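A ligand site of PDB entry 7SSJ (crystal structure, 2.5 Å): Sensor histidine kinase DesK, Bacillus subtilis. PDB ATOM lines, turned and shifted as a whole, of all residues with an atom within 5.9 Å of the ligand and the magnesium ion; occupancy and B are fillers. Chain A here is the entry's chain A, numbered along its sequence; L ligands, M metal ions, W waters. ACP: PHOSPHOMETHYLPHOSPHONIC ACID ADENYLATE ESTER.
NZ of Lys 150 lies within salt-bridge range of O2G of the ligand.
N of Leu 191 lies within hydrogen-bond range of O2A of the ligand, at 3.0 Å.
The backbone NH of Gly 180 lies within hydrogen-bond range of an oxygen (O2') of the ligand.
The backbone NH (N) of Lys 179 is in hydrogen-bond range of a nitrogen (N3) of the ligand (3.0 Å).
A ring nitrogen (ND1) of His 189 lies within hydrogen-bond range of an oxygen (O3A) of the ligand.
OD2 of Asp 174 is in hydrogen-bond range of N6 of the ligand (3.0 Å).
NE2 of His 151 sits close to O2B of the ligand, 2.9 Å away.
An oxygen (O2') of the ligand lies close to the backbone carbonyl oxygen of Lys 179 (3.3 Å).
The backbone NH (N) of Gly 190 lies within hydrogen-bond range of an oxygen (O2A) of the ligand, 3.3 Å away.
NZ of Lys 179 sits at hydrogen-bond distance from O of His 151.
O of Val 148 lies within hydrogen-bond range of OG of Ser 152, 2.4 Å away.
N of Asp 174 lies within hydrogen-bond range of O of Thr 213 (3.1 Å).
OG of Ser 184 lies within hydrogen-bond range of N of Glu 181 (3.4 Å).
N of Thr 177 is in hydrogen-bond range of O of Ser 152.
A ring nitrogen (ND1) of His 189 sits close to the side-chain hydroxyl of Ser 186 (3.2 Å).
Residues that only touch the ligand: Thr 177 (3.2 Å), Phe 178 (3.4 Å), Ser 152 (3.5 Å), Gly 188 (3.6 Å), Ser 184 (3.7 Å) and Thr 213 (3.8 Å).
Hydrophobic or aromatic side chains within 4 Å of the ligand: His 151, Phe 178, His 189 and Leu 191.
Of the 24 residues printed, 16 come within 4 Å of the ligand.
Along chain A the residues within 4 Å of the ligand span positions 143 to 213.
Within 4 Å of the magnesium ion: Glu 143 and Asn 147.
Along chain A the residues within 4 Å of the magnesium ion span positions 143 to 147.
The nearest printed residue that does not touch the magnesium ion is Gly 190 (4.3 Å).
The magnesium ion is bound by O3G of the ligand (2.0 Å), OE2 of Glu 143 (2.0 Å), O1A of the ligand (2.1 Å), OD1 of Asn 147 (2.1 Å), O2B of the ligand (2.1 Å) and water W1 (2.2 Å).
The magnesium ion has six donor atoms within binding distance.
Water W1 lies within hydrogen-bond range of NZ of Lys 150 (3.0 Å), OE1 of Glu 143 (3.3 Å) and O2G of the ligand (3.4 Å).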
ATOM      1  N   GLU A 143      16.695   5.498  10.051  1.00  0.00           N
ATOM      2  CA  GLU A 143      17.354   6.686   9.523  1.00  0.00           C
ATOM      3  C   GLU A 143      16.382   7.562   8.765  1.00  0.00           C
ATOM      4  O   GLU A 143      16.447   8.787   8.898  1.00  0.00           O
ATOM      5  CB  GLU A 143      18.582   6.311   8.669  1.00  0.00           C
ATOM      6  CG  GLU A 143      19.296   7.490   8.042  1.00  0.00           C
ATOM      7  CD  GLU A 143      19.755   8.596   8.966  1.00  0.00           C
ATOM      8  OE1 GLU A 143      19.925   8.340  10.183  1.00  0.00           O
ATOM      9  OE2 GLU A 143      19.939   9.729   8.478  1.00  0.00           O
ATOM     10  N   ALA A 144      15.427   6.952   8.039  1.00  0.00           N
ATOM     11  CA  ALA A 144      14.408   7.689   7.303  1.00  0.00           C
ATOM     12  C   ALA A 144      13.575   8.578   8.238  1.00  0.00           C
ATOM     13  O   ALA A 144      13.504   9.775   7.988  1.00  0.00           O
ATOM     14  CB  ALA A 144      13.520   6.730   6.537  1.00  0.00           C
ATOM     15  N   THR A 146      14.429   9.558  11.295  1.00  0.00           N
ATOM     16  CA  THR A 146      15.359  10.481  11.957  1.00  0.00           C
ATOM     17  C   THR A 146      15.518  11.732  11.079  1.00  0.00           C
ATOM     18  O   THR A 146      15.502  12.860  11.589  1.00  0.00           O
ATOM     19  CB  THR A 146      16.686   9.769  12.207  1.00  0.00           C
ATOM     20  OG1 THR A 146      16.430   8.706  13.104  1.00  0.00           O
ATOM     21  CG2 THR A 146      17.748  10.693  12.776  1.00  0.00           C
ATOM     22  N   ASN A 147      15.633  11.539   9.760  1.00  0.00           N
ATOM     23  CA  ASN A 147      15.726  12.636   8.840  1.00  0.00           C
ATOM     24  C   ASN A 147      14.428  13.435   8.814  1.00  0.00           C
ATOM     25  O   ASN A 147      14.492  14.650   8.683  1.00  0.00           O
ATOM     26  CB  ASN A 147      16.064  12.129   7.453  1.00  0.00           C
ATOM     27  CG  ASN A 147      17.505  11.713   7.290  1.00  0.00           C
ATOM     28  OD1 ASN A 147      18.320  11.780   8.226  1.00  0.00           O
ATOM     29  ND2 ASN A 147      17.838  11.304   6.097  1.00  0.00           N
ATOM     30  N   VAL A 148      13.267  12.766   8.947  1.00  0.00           N
ATOM     31  CA  VAL A 148      12.000  13.482   8.913  1.00  0.00           C
ATOM     32  C   VAL A 148      11.794  14.297  10.202  1.00  0.00           C
ATOM     33  O   VAL A 148      11.130  15.333  10.135  1.00  0.00           O
ATOM     34  CB  VAL A 148      10.715  12.662   8.497  1.00  0.00           C
ATOM     35  CG1 VAL A 148      11.047  11.439   7.668  1.00  0.00           C
ATOM     36  CG2 VAL A 148       9.806  12.317   9.661  1.00  0.00           C
ATOM     37  N   LYS A 150      14.288  15.727  12.042  1.00  0.00           N
ATOM     38  CA  LYS A 150      15.262  16.816  12.052  1.00  0.00           C
ATOM     39  C   LYS A 150      15.125  17.843  10.950  1.00  0.00           C
ATOM     40  O   LYS A 150      15.413  19.005  11.187  1.00  0.00           O
ATOM     41  CB  LYS A 150      16.699  16.255  12.023  1.00  0.00           C
ATOM     42  CG  LYS A 150      16.976  15.163  13.043  1.00  0.00           C
ATOM     43  CD  LYS A 150      18.477  14.878  13.162  1.00  0.00           C
ATOM     44  CE  LYS A 150      19.168  14.520  11.871  1.00  0.00           C
ATOM     45  NZ  LYS A 150      20.589  14.127  12.094  1.00  0.00           N
ATOM     46  N   HIS A 151      14.773  17.410   9.730  1.00  0.00           N
ATOM     47  CA  HIS A 151      14.770  18.319   8.580  1.00  0.00           C
ATOM     48  C   HIS A 151      13.439  18.591   7.903  1.00  0.00           C
ATOM     49  O   HIS A 151      13.240  19.697   7.424  1.00  0.00           O
ATOM     50  CB  HIS A 151      15.736  17.844   7.490  1.00  0.00           C
ATOM     51  CG  HIS A 151      16.933  17.081   7.959  1.00  0.00           C
ATOM     52  ND1 HIS A 151      17.921  17.679   8.726  1.00  0.00           N
ATOM     53  CD2 HIS A 151      17.293  15.804   7.700  1.00  0.00           C
ATOM     54  CE1 HIS A 151      18.831  16.748   8.919  1.00  0.00           C
ATOM     55  NE2 HIS A 151      18.498  15.606   8.330  1.00  0.00           N
ATOM     56  N   SER A 152      12.599  17.583   7.729  1.00  0.00           N
ATOM     57  CA  SER A 152      11.383  17.708   6.938  1.00  0.00           C
ATOM     58  C   SER A 152      10.455  18.874   7.268  1.00  0.00           C
ATOM     59  O   SER A 152       9.992  19.543   6.338  1.00  0.00           O
ATOM     60  CB  SER A 152      10.581  16.418   6.983  1.00  0.00           C
ATOM     61  OG  SER A 152       9.946  16.269   8.245  1.00  0.00           O
ATOM     62  N   ASP A 174       7.081  11.897   3.889  1.00  0.00           N
ATOM     63  CA  ASP A 174       6.694  13.000   4.752  1.00  0.00           C
ATOM     64  C   ASP A 174       6.152  14.164   3.889  1.00  0.00           C
ATOM     65  O   ASP A 174       6.535  14.317   2.716  1.00  0.00           O
ATOM     66  CB  ASP A 174       7.862  13.459   5.652  1.00  0.00           C
ATOM     67  CG  ASP A 174       9.073  13.978   4.886  1.00  0.00           C
ATOM     68  OD1 ASP A 174       9.015  15.146   4.401  1.00  0.00           O
ATOM     69  OD2 ASP A 174      10.079  13.228   4.783  1.00  0.00           O
ATOM     70  N   THR A 177       9.361  19.634   3.434  1.00  0.00           N
ATOM     71  CA  THR A 177      10.139  20.117   2.280  1.00  0.00           C
ATOM     72  C   THR A 177      11.557  19.571   2.353  1.00  0.00           C
ATOM     73  O   THR A 177      12.139  19.556   3.439  1.00  0.00           O
ATOM     74  CB  THR A 177      10.104  21.649   2.153  1.00  0.00           C
ATOM     75  OG1 THR A 177      10.215  22.243   3.452  1.00  0.00           O
ATOM     76  CG2 THR A 177       8.838  22.148   1.497  1.00  0.00           C
ATOM     77  N   PHE A 178      12.107  19.097   1.223  1.00  0.00           N
ATOM     78  CA  PHE A 178      13.467  18.540   1.201  1.00  0.00           C
ATOM     79  C   PHE A 178      14.533  19.630   1.336  1.00  0.00           C
ATOM     80  O   PHE A 178      14.673  20.468   0.447  1.00  0.00           O
ATOM     81  CB  PHE A 178      13.692  17.671  -0.044  1.00  0.00           C
ATOM     82  CG  PHE A 178      14.968  16.889   0.003  1.00  0.00           C
ATOM     83  CD1 PHE A 178      15.099  15.789   0.823  1.00  0.00           C
ATOM     84  CD2 PHE A 178      16.042  17.252  -0.798  1.00  0.00           C
ATOM     85  CE1 PHE A 178      16.282  15.071   0.853  1.00  0.00           C
ATOM     86  CE2 PHE A 178      17.224  16.533  -0.757  1.00  0.00           C
ATOM     87  CZ  PHE A 178      17.340  15.459   0.075  1.00  0.00           C
ATOM     88  N   LYS A 179      15.261  19.622   2.460  1.00  0.00           N
ATOM     89  CA  LYS A 179      16.262  20.643   2.795  1.00  0.00           C
ATOM     90  C   LYS A 179      17.650  20.434   2.202  1.00  0.00           C
ATOM     91  O   LYS A 179      18.526  21.271   2.438  1.00  0.00           O
ATOM     92  CB  LYS A 179      16.378  20.819   4.315  1.00  0.00           C
ATOM     93  CG  LYS A 179      15.042  20.971   5.035  1.00  0.00           C
ATOM     94  CD  LYS A 179      14.251  22.192   4.591  1.00  0.00           C
ATOM     95  CE  LYS A 179      12.848  22.199   5.148  1.00  0.00           C
ATOM     96  NZ  LYS A 179      12.809  22.522   6.588  1.00  0.00           N
ATOM     97  N   GLY A 180      17.861  19.337   1.483  1.00  0.00           N
ATOM     98  CA  GLY A 180      19.146  19.005   0.879  1.00  0.00           C
ATOM     99  C   GLY A 180      19.595  20.006  -0.166  1.00  0.00           C
ATOM    100  O   GLY A 180      18.789  20.792  -0.664  1.00  0.00           O
ATOM    101  N   GLU A 181      20.897  20.034  -0.442  1.00  0.00           N
ATOM    102  CA  GLU A 181      21.454  21.025  -1.373  1.00  0.00           C
ATOM    103  C   GLU A 181      22.454  20.403  -2.359  1.00  0.00           C
ATOM    104  O   GLU A 181      23.637  20.275  -2.024  1.00  0.00           O
ATOM    105  CB  GLU A 181      22.117  22.195  -0.582  1.00  0.00           C
ATOM    106  CG  GLU A 181      21.240  22.823   0.500  1.00  0.00           C
ATOM    107  CD  GLU A 181      21.189  24.341   0.543  1.00  0.00           C
ATOM    108  OE1 GLU A 181      20.571  24.947  -0.372  1.00  0.00           O
ATOM    109  OE2 GLU A 181      21.736  24.925   1.498  1.00  0.00           O
ATOM    110  N   SER A 184      23.176  15.901  -1.906  1.00  0.00           N
ATOM    111  CA  SER A 184      22.464  15.471  -0.692  1.00  0.00           C
ATOM    112  C   SER A 184      22.954  14.112  -0.128  1.00  0.00           C
ATOM    113  O   SER A 184      22.512  13.686   0.938  1.00  0.00           O
ATOM    114  CB  SER A 184      20.961  15.470  -0.927  1.00  0.00           C
ATOM    115  OG  SER A 184      20.522  16.791  -1.231  1.00  0.00           O
ATOM    116  N   PHE A 185      23.905  13.477  -0.835  1.00  0.00           N
ATOM    117  CA  PHE A 185      24.587  12.235  -0.480  1.00  0.00           C
ATOM    118  C   PHE A 185      26.028  12.556  -0.138  1.00  0.00           C
ATOM    119  O   PHE A 185      26.939  12.278  -0.925  1.00  0.00           O
ATOM    120  CB  PHE A 185      24.514  11.220  -1.647  1.00  0.00           C
ATOM    121  CG  PHE A 185      23.222  10.437  -1.664  1.00  0.00           C
ATOM    122  CD1 PHE A 185      22.020  11.051  -1.960  1.00  0.00           C
ATOM    123  CD2 PHE A 185      23.202   9.082  -1.367  1.00  0.00           C
ATOM    124  CE1 PHE A 185      20.838  10.339  -1.954  1.00  0.00           C
ATOM    125  CE2 PHE A 185      22.020   8.370  -1.360  1.00  0.00           C
ATOM    126  CZ  PHE A 185      20.838   9.005  -1.643  1.00  0.00           C
ATOM    127  N   SER A 186      26.244  13.183   1.028  1.00  0.00           N
ATOM    128  CA  SER A 186      27.579  13.543   1.490  1.00  0.00           C
ATOM    129  C   SER A 186      28.260  12.387   2.260  1.00  0.00           C
ATOM    130  O   SER A 186      27.571  11.453   2.687  1.00  0.00           O
ATOM    131  CB  SER A 186      27.565  14.841   2.304  1.00  0.00           C
ATOM    132  OG  SER A 186      26.462  14.893   3.205  1.00  0.00           O
ATOM    133  N   GLY A 188      29.891   9.946   4.915  1.00  0.00           N
ATOM    134  CA  GLY A 188      29.566   9.591   6.298  1.00  0.00           C
ATOM    135  C   GLY A 188      28.168   9.975   6.741  1.00  0.00           C
ATOM    136  O   GLY A 188      27.872   9.986   7.938  1.00  0.00           O
ATOM    137  N   HIS A 189      27.289  10.278   5.797  1.00  0.00           N
ATOM    138  CA  HIS A 189      25.912  10.680   6.092  1.00  0.00           C
ATOM    139  C   HIS A 189      24.937   9.523   6.004  1.00  0.00           C
ATOM    140  O   HIS A 189      25.303   8.442   5.546  1.00  0.00           O
ATOM    141  CB  HIS A 189      25.505  11.870   5.229  1.00  0.00           C
ATOM    142  CG  HIS A 189      25.963  13.176   5.794  1.00  0.00           C
ATOM    143  ND1 HIS A 189      25.094  14.225   5.991  1.00  0.00           N
ATOM    144  CD2 HIS A 189      27.193  13.528   6.240  1.00  0.00           C
ATOM    145  CE1 HIS A 189      25.824  15.192   6.529  1.00  0.00           C
ATOM    146  NE2 HIS A 189      27.091  14.817   6.696  1.00  0.00           N
ATOM    147  N   GLY A 190      23.744   9.726   6.515  1.00  0.00           N
ATOM    148  CA  GLY A 190      22.730   8.693   6.571  1.00  0.00           C
ATOM    149  C   GLY A 190      22.230   8.199   5.235  1.00  0.00           C
ATOM    150  O   GLY A 190      22.060   6.997   5.060  1.00  0.00           O
ATOM    151  N   LEU A 191      21.981   9.110   4.296  1.00  0.00           N
ATOM    152  CA  LEU A 191      21.477   8.729   2.974  1.00  0.00           C
ATOM    153  C   LEU A 191      22.471   7.912   2.186  1.00  0.00           C
ATOM    154  O   LEU A 191      22.098   6.887   1.619  1.00  0.00           O
ATOM    155  CB  LEU A 191      20.996   9.952   2.172  1.00  0.00           C
ATOM    156  CG  LEU A 191      19.703  10.576   2.659  1.00  0.00           C
ATOM    157  CD1 LEU A 191      19.389  11.814   1.888  1.00  0.00           C
ATOM    158  CD2 LEU A 191      18.568   9.600   2.565  1.00  0.00           C
ATOM    159  N   LEU A 192      23.743   8.340   2.190  1.00  0.00           N
ATOM    160  CA  LEU A 192      24.807   7.602   1.526  1.00  0.00           C
ATOM    161  C   LEU A 192      25.005   6.209   2.132  1.00  0.00           C
ATOM    162  O   LEU A 192      25.149   5.218   1.412  1.00  0.00           O
ATOM    163  CB  LEU A 192      26.117   8.402   1.587  1.00  0.00           C
ATOM    164  CG  LEU A 192      27.293   7.726   0.916  1.00  0.00           C
ATOM    165  CD1 LEU A 192      27.076   7.572  -0.576  1.00  0.00           C
ATOM    166  CD2 LEU A 192      28.599   8.429   1.247  1.00  0.00           C
ATOM    167  N   THR A 213       8.920  14.397   0.381  1.00  0.00           N
ATOM    168  CA  THR A 213      10.077  13.497   0.318  1.00  0.00           C
ATOM    169  C   THR A 213       9.585  12.062   0.461  1.00  0.00           C
ATOM    170  O   THR A 213       8.911  11.747   1.439  1.00  0.00           O
ATOM    171  CB  THR A 213      11.155  13.834   1.380  1.00  0.00           C
ATOM    172  OG1 THR A 213      11.614  15.192   1.225  1.00  0.00           O
ATOM    173  CG2 THR A 213      12.355  12.878   1.321  1.00  0.00           C
ATOM    174  N   LEU A 215      11.017   8.180   0.318  1.00  0.00           N
ATOM    175  CA  LEU A 215      12.120   7.225   0.225  1.00  0.00           C
ATOM    176  C   LEU A 215      11.599   5.847  -0.050  1.00  0.00           C
ATOM    177  O   LEU A 215      10.708   5.394   0.658  1.00  0.00           O
ATOM    178  CB  LEU A 215      12.961   7.238   1.498  1.00  0.00           C
ATOM    179  CG  LEU A 215      14.274   7.980   1.391  1.00  0.00           C
ATOM    180  CD1 LEU A 215      14.054   9.468   1.169  1.00  0.00           C
ATOM    181  CD2 LEU A 215      15.064   7.810   2.629  1.00  0.00           C
HETATM  182  PG  ACP L   1      23.573  12.081   9.629  1.00  0.00           P
HETATM  183  O1G ACP L   1      24.828  11.542   9.019  1.00  0.00           O
HETATM  184  O2G ACP L   1      23.569  11.924  11.163  1.00  0.00           O
HETATM  185  O3G ACP L   1      22.314  11.368   9.097  1.00  0.00           O
HETATM  186  PB  ACP L   1      22.127  14.361   8.112  1.00  0.00           P
HETATM  187  O1B ACP L   1      22.008  15.855   7.866  1.00  0.00           O
HETATM  188  O2B ACP L   1      20.753  13.818   8.624  1.00  0.00           O
HETATM  189  C3B ACP L   1      23.366  13.838   9.309  1.00  0.00           C
HETATM  190  PA  ACP L   1      21.507  12.780   5.720  1.00  0.00           P
HETATM  191  O1A ACP L   1      20.670  11.798   6.447  1.00  0.00           O
HETATM  192  O2A ACP L   1      22.389  12.078   4.719  1.00  0.00           O
HETATM  193  O3A ACP L   1      22.443  13.551   6.748  1.00  0.00           O
HETATM  194  O5' ACP L   1      20.658  13.888   4.957  1.00  0.00           O
HETATM  195  C5' ACP L   1      21.396  14.867   4.225  1.00  0.00           C
HETATM  196  C4' ACP L   1      20.539  16.098   4.092  1.00  0.00           C
HETATM  197  O4' ACP L   1      19.391  15.800   3.283  1.00  0.00           O
HETATM  198  C3' ACP L   1      19.950  16.636   5.400  1.00  0.00           C
HETATM  199  O3' ACP L   1      20.872  17.443   6.128  1.00  0.00           O
HETATM  200  C2' ACP L   1      18.754  17.432   4.894  1.00  0.00           C
HETATM  201  O2' ACP L   1      19.214  18.671   4.362  1.00  0.00           O
HETATM  202  C1' ACP L   1      18.267  16.532   3.741  1.00  0.00           C
HETATM  203  N9  ACP L   1      17.199  15.608   4.111  1.00  0.00           N
HETATM  204  C8  ACP L   1      17.291  14.249   4.292  1.00  0.00           C
HETATM  205  N7  ACP L   1      16.157  13.656   4.568  1.00  0.00           N
HETATM  206  C5  ACP L   1      15.235  14.693   4.559  1.00  0.00           C
HETATM  207  C6  ACP L   1      13.832  14.743   4.698  1.00  0.00           C
HETATM  208  N6  ACP L   1      13.083  13.682   4.986  1.00  0.00           N
HETATM  209  N1  ACP L   1      13.218  15.927   4.541  1.00  0.00           N
HETATM  210  C2  ACP L   1      13.965  17.013   4.276  1.00  0.00           C
HETATM  211  N3  ACP L   1      15.295  17.105   4.130  1.00  0.00           N
HETATM  212  C4  ACP L   1      15.874  15.914   4.275  1.00  0.00           C
HETATM  213 MG    MG M   1      20.402  11.703   8.530  1.00  0.00          MG
HETATM  214  O   HOH W   1      20.195  11.566  10.672  1.00  0.00           O
